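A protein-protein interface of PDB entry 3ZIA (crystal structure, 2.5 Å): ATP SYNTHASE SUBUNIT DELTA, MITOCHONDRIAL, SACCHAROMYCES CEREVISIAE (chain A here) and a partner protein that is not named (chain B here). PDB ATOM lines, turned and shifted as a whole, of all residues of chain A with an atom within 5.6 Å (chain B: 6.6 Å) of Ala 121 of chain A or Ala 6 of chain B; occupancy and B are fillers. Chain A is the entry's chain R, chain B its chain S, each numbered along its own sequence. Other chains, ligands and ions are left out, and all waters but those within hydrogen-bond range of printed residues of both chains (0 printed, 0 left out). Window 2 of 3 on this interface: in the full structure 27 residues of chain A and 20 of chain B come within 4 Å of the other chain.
Ala 6 of chain B touches Ala 121 of chain A.
Ala 124 of chain A touches Ser 1 of chain B.
Ile 125 of chain A touches Ser 1 of chain B.
Ile 125 of chain A touches Trp 3 of chain B.
The guanidinium group (NE) of Arg 118 of chain A is in salt-bridge range of the side-chain carboxylate (OE2) of Glu 122 of chain A, 3.2 Å away.
The backbone NH (N) of Ile 8 of chain B sits at hydrogen-bond distance from the backbone carbonyl oxygen (O) of Trp 3 of chain B (3.4 Å).
Of the printed residues of chain B, Arg 118 of chain A touches Gly 7 and Ile 8.
Ala 120 of chain A touches none of the printed residues of chain B.
Ala 121 of chain A touches one residue of chain B.
Of the printed residues of chain A, Ser 1 of chain B touches Ala 124 (3.9 Å) and Ile 125 (3.9 Å).
Printed residues of chain A within 4 Å of Trp 3 of chain B: Ile 125 (3.998 Å).
Arg 4 of chain B touches none of the printed residues of chain A.
Of the printed residues of chain A, Ala 6 of chain B touches Ala 121.
Of the printed residues of chain A, Ile 8 of chain B touches Arg 118.
The nearest residue of chain A that does not touch Ala 6 of chain B is Arg 118 of chain A (4.2 Å).
Of the 10 printed residues of chain A, 4 touch a printed residue of chain B.
Hydrophobic or aromatic side chains of chain A within 4 Å of the printed part of chain B: Ala 121 and Ile 125.
Of the 9 printed residues of chain B, 5 touch a printed residue of chain A.
Hydrophobic or aromatic side chains of chain B within 4 Å of the printed part of chain A: Trp 3, Ala 6 and Ile 8.
NH1 of Arg 118 of chain A lies close to O of Gly 7 of chain B (3.5 Å).
The backbone NH of Ile 8 of chain B sits close to the guanidinium group of Arg 118 of chain A.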
ATOM      1  N   ASN A 111     -27.576 -33.151 -27.985  1.00  0.00           N
ATOM      2  CA  ASN A 111     -27.788 -32.590 -26.656  1.00  0.00           C
ATOM      3  C   ASN A 111     -28.452 -31.210 -26.632  1.00  0.00           C
ATOM      4  O   ASN A 111     -29.023 -30.822 -25.611  1.00  0.00           O
ATOM      5  CB  ASN A 111     -26.492 -32.612 -25.831  1.00  0.00           C
ATOM      6  CG  ASN A 111     -26.212 -33.975 -25.218  1.00  0.00           C
ATOM      7  OD1 ASN A 111     -27.132 -34.694 -24.827  1.00  0.00           O
ATOM      8  ND2 ASN A 111     -24.934 -34.333 -25.126  1.00  0.00           N
ATOM      9  N   ALA A 117     -32.934 -27.852 -18.456  1.00  0.00           N
ATOM     10  CA  ALA A 117     -31.632 -27.532 -17.862  1.00  0.00           C
ATOM     11  C   ALA A 117     -30.732 -26.789 -18.836  1.00  0.00           C
ATOM     12  O   ALA A 117     -31.065 -26.583 -20.010  1.00  0.00           O
ATOM     13  CB  ALA A 117     -30.913 -28.791 -17.309  1.00  0.00           C
ATOM     14  N   ARG A 118     -29.584 -26.381 -18.316  1.00  0.00           N
ATOM     15  CA  ARG A 118     -28.540 -25.811 -19.125  1.00  0.00           C
ATOM     16  C   ARG A 118     -27.715 -26.912 -19.779  1.00  0.00           C
ATOM     17  O   ARG A 118     -26.825 -26.626 -20.577  1.00  0.00           O
ATOM     18  CB  ARG A 118     -27.677 -24.879 -18.287  1.00  0.00           C
ATOM     19  CG  ARG A 118     -26.691 -25.529 -17.334  1.00  0.00           C
ATOM     20  CD  ARG A 118     -25.593 -24.525 -17.194  1.00  0.00           C
ATOM     21  NE  ARG A 118     -24.686 -24.695 -16.072  1.00  0.00           N
ATOM     22  CZ  ARG A 118     -24.044 -23.679 -15.504  1.00  0.00           C
ATOM     23  NH1 ARG A 118     -24.239 -22.447 -15.937  1.00  0.00           N
ATOM     24  NH2 ARG A 118     -23.222 -23.884 -14.491  1.00  0.00           N
ATOM     25  N   GLU A 119     -28.013 -28.165 -19.435  1.00  0.00           N
ATOM     26  CA  GLU A 119     -27.511 -29.306 -20.194  1.00  0.00           C
ATOM     27  C   GLU A 119     -27.818 -29.036 -21.661  1.00  0.00           C
ATOM     28  O   GLU A 119     -26.952 -29.201 -22.523  1.00  0.00           O
ATOM     29  CB  GLU A 119     -28.181 -30.612 -19.750  1.00  0.00           C
ATOM     30  CG  GLU A 119     -27.635 -31.857 -20.464  1.00  0.00           C
ATOM     31  CD  GLU A 119     -28.648 -32.994 -20.566  1.00  0.00           C
ATOM     32  OE1 GLU A 119     -29.834 -32.737 -20.882  1.00  0.00           O
ATOM     33  OE2 GLU A 119     -28.249 -34.156 -20.344  1.00  0.00           O
ATOM     34  N   ALA A 120     -29.053 -28.598 -21.917  1.00  0.00           N
ATOM     35  CA  ALA A 120     -29.504 -28.189 -23.246  1.00  0.00           C
ATOM     36  C   ALA A 120     -28.694 -27.006 -23.770  1.00  0.00           C
ATOM     37  O   ALA A 120     -28.260 -27.003 -24.926  1.00  0.00           O
ATOM     38  CB  ALA A 120     -30.991 -27.849 -23.218  1.00  0.00           C
ATOM     39  N   ALA A 121     -28.482 -26.014 -22.907  1.00  0.00           N
ATOM     40  CA  ALA A 121     -27.790 -24.778 -23.283  1.00  0.00           C
ATOM     41  C   ALA A 121     -26.275 -24.944 -23.461  1.00  0.00           C
ATOM     42  O   ALA A 121     -25.672 -24.270 -24.299  1.00  0.00           O
ATOM     43  CB  ALA A 121     -28.096 -23.680 -22.277  1.00  0.00           C
ATOM     44  N   GLU A 122     -25.673 -25.833 -22.670  1.00  0.00           N
ATOM     45  CA  GLU A 122     -24.236 -26.116 -22.751  1.00  0.00           C
ATOM     46  C   GLU A 122     -23.874 -26.750 -24.089  1.00  0.00           C
ATOM     47  O   GLU A 122     -22.832 -26.438 -24.670  1.00  0.00           O
ATOM     48  CB  GLU A 122     -23.784 -27.026 -21.596  1.00  0.00           C
ATOM     49  CG  GLU A 122     -23.241 -26.286 -20.368  1.00  0.00           C
ATOM     50  CD  GLU A 122     -23.059 -27.181 -19.142  1.00  0.00           C
ATOM     51  OE1 GLU A 122     -22.911 -28.414 -19.294  1.00  0.00           O
ATOM     52  OE2 GLU A 122     -23.062 -26.641 -18.015  1.00  0.00           O
ATOM     53  N   ALA A 123     -24.743 -27.638 -24.565  1.00  0.00           N
ATOM     54  CA  ALA A 123     -24.569 -28.292 -25.859  1.00  0.00           C
ATOM     55  C   ALA A 123     -24.505 -27.265 -26.978  1.00  0.00           C
ATOM     56  O   ALA A 123     -23.621 -27.330 -27.838  1.00  0.00           O
ATOM     57  CB  ALA A 123     -25.688 -29.266 -26.105  1.00  0.00           C
ATOM     58  N   ALA A 124     -25.437 -26.312 -26.950  1.00  0.00           N
ATOM     59  CA  ALA A 124     -25.479 -25.220 -27.920  1.00  0.00           C
ATOM     60  C   ALA A 124     -24.127 -24.521 -28.035  1.00  0.00           C
ATOM     61  O   ALA A 124     -23.701 -24.151 -29.129  1.00  0.00           O
ATOM     62  CB  ALA A 124     -26.578 -24.223 -27.553  1.00  0.00           C
ATOM     63  N   ILE A 125     -23.454 -24.364 -26.896  1.00  0.00           N
ATOM     64  CA  ILE A 125     -22.145 -23.725 -26.838  1.00  0.00           C
ATOM     65  C   ILE A 125     -21.087 -24.593 -27.510  1.00  0.00           C
ATOM     66  O   ILE A 125     -20.208 -24.083 -28.202  1.00  0.00           O
ATOM     67  CB  ILE A 125     -21.738 -23.415 -25.380  1.00  0.00           C
ATOM     68  CG1 ILE A 125     -22.793 -22.510 -24.720  1.00  0.00           C
ATOM     69  CG2 ILE A 125     -20.347 -22.787 -25.335  1.00  0.00           C
ATOM     70  CD1 ILE A 125     -22.741 -22.470 -23.200  1.00  0.00           C
ATOM     71  N   SER B   1     -23.411 -17.575 -28.283  1.00  0.00           N
ATOM     72  CA  SER B   1     -24.703 -18.255 -27.969  1.00  0.00           C
ATOM     73  C   SER B   1     -25.531 -17.459 -26.944  1.00  0.00           C
ATOM     74  O   SER B   1     -25.314 -16.258 -26.761  1.00  0.00           O
ATOM     75  CB  SER B   1     -24.447 -19.686 -27.473  1.00  0.00           C
ATOM     76  OG  SER B   1     -23.543 -20.376 -28.324  1.00  0.00           O
ATOM     77  N   ALA B   2     -26.470 -18.133 -26.283  1.00  0.00           N
ATOM     78  CA  ALA B   2     -27.353 -17.488 -25.310  1.00  0.00           C
ATOM     79  C   ALA B   2     -27.265 -18.113 -23.912  1.00  0.00           C
ATOM     80  O   ALA B   2     -28.291 -18.457 -23.310  1.00  0.00           O
ATOM     81  CB  ALA B   2     -28.795 -17.493 -25.818  1.00  0.00           C
ATOM     82  N   TRP B   3     -26.042 -18.246 -23.395  1.00  0.00           N
ATOM     83  CA  TRP B   3     -25.828 -18.735 -22.029  1.00  0.00           C
ATOM     84  C   TRP B   3     -26.338 -17.742 -20.982  1.00  0.00           C
ATOM     85  O   TRP B   3     -26.361 -18.021 -19.783  1.00  0.00           O
ATOM     86  CB  TRP B   3     -24.357 -19.093 -21.798  1.00  0.00           C
ATOM     87  CG  TRP B   3     -23.335 -17.985 -21.992  1.00  0.00           C
ATOM     88  CD1 TRP B   3     -22.936 -17.052 -21.068  1.00  0.00           C
ATOM     89  CD2 TRP B   3     -22.550 -17.745 -23.166  1.00  0.00           C
ATOM     90  NE1 TRP B   3     -21.966 -16.236 -21.607  1.00  0.00           N
ATOM     91  CE2 TRP B   3     -21.711 -16.639 -22.892  1.00  0.00           C
ATOM     92  CE3 TRP B   3     -22.480 -18.351 -24.426  1.00  0.00           C
ATOM     93  CZ2 TRP B   3     -20.814 -16.127 -23.835  1.00  0.00           C
ATOM     94  CZ3 TRP B   3     -21.592 -17.838 -25.362  1.00  0.00           C
ATOM     95  CH2 TRP B   3     -20.771 -16.738 -25.061  1.00  0.00           C
ATOM     96  N   ARG B   4     -26.767 -16.589 -21.486  1.00  0.00           N
ATOM     97  CA  ARG B   4     -27.312 -15.490 -20.704  1.00  0.00           C
ATOM     98  C   ARG B   4     -28.620 -15.906 -20.038  1.00  0.00           C
ATOM     99  O   ARG B   4     -28.757 -15.804 -18.818  1.00  0.00           O
ATOM    100  CB  ARG B   4     -27.536 -14.258 -21.605  1.00  0.00           C
ATOM    101  CG  ARG B   4     -26.723 -14.209 -22.936  1.00  0.00           C
ATOM    102  CD  ARG B   4     -25.253 -14.658 -22.804  1.00  0.00           C
ATOM    103  NE  ARG B   4     -24.615 -14.151 -21.587  1.00  0.00           N
ATOM    104  CZ  ARG B   4     -23.598 -13.296 -21.564  1.00  0.00           C
ATOM    105  NH1 ARG B   4     -23.068 -12.846 -22.697  1.00  0.00           N
ATOM    106  NH2 ARG B   4     -23.099 -12.899 -20.400  1.00  0.00           N
ATOM    107  N   LYS B   5     -29.573 -16.379 -20.849  1.00  0.00           N
ATOM    108  CA  LYS B   5     -30.869 -16.873 -20.355  1.00  0.00           C
ATOM    109  C   LYS B   5     -30.651 -18.030 -19.381  1.00  0.00           C
ATOM    110  O   LYS B   5     -31.256 -18.078 -18.304  1.00  0.00           O
ATOM    111  CB  LYS B   5     -31.777 -17.328 -21.514  1.00  0.00           C
ATOM    112  CG  LYS B   5     -31.719 -16.462 -22.778  1.00  0.00           C
ATOM    113  CD  LYS B   5     -32.417 -15.121 -22.610  1.00  0.00           C
ATOM    114  CE  LYS B   5     -31.805 -14.097 -23.550  1.00  0.00           C
ATOM    115  NZ  LYS B   5     -32.839 -13.201 -24.126  1.00  0.00           N
ATOM    116  N   ALA B   6     -29.774 -18.952 -19.775  1.00  0.00           N
ATOM    117  CA  ALA B   6     -29.339 -20.047 -18.923  1.00  0.00           C
ATOM    118  C   ALA B   6     -28.472 -19.516 -17.781  1.00  0.00           C
ATOM    119  O   ALA B   6     -28.119 -18.336 -17.756  1.00  0.00           O
ATOM    120  CB  ALA B   6     -28.580 -21.064 -19.745  1.00  0.00           C
ATOM    121  N   GLY B   7     -28.129 -20.389 -16.840  1.00  0.00           N
ATOM    122  CA  GLY B   7     -27.348 -19.982 -15.670  1.00  0.00           C
ATOM    123  C   GLY B   7     -25.868 -19.685 -15.891  1.00  0.00           C
ATOM    124  O   GLY B   7     -25.185 -19.277 -14.947  1.00  0.00           O
ATOM    125  N   ILE B   8     -25.380 -19.863 -17.127  1.00  0.00           N
ATOM    126  CA  ILE B   8     -23.929 -19.857 -17.432  1.00  0.00           C
ATOM    127  C   ILE B   8     -23.211 -18.520 -17.233  1.00  0.00           C
ATOM    128  O   ILE B   8     -23.656 -17.475 -17.713  1.00  0.00           O
ATOM    129  CB  ILE B   8     -23.591 -20.442 -18.852  1.00  0.00           C
ATOM    130  CG1 ILE B   8     -23.861 -21.943 -18.928  1.00  0.00           C
ATOM    131  CG2 ILE B   8     -22.129 -20.241 -19.211  1.00  0.00           C
ATOM    132  CD1 ILE B   8     -25.195 -22.302 -19.527  1.00  0.00           C
ATOM    133  N   SER B   9     -22.092 -18.590 -16.515  1.00  0.00           N
ATOM    134  CA  SER B   9     -21.196 -17.466 -16.306  1.00  0.00           C
ATOM    135  C   SER B   9     -20.105 -17.491 -17.369  1.00  0.00           C
ATOM    136  O   SER B   9     -19.930 -18.493 -18.057  1.00  0.00           O
ATOM    137  CB  SER B   9     -20.574 -17.553 -14.915  1.00  0.00           C
ATOM    138  OG  SER B   9     -19.797 -18.732 -14.782  1.00  0.00           O
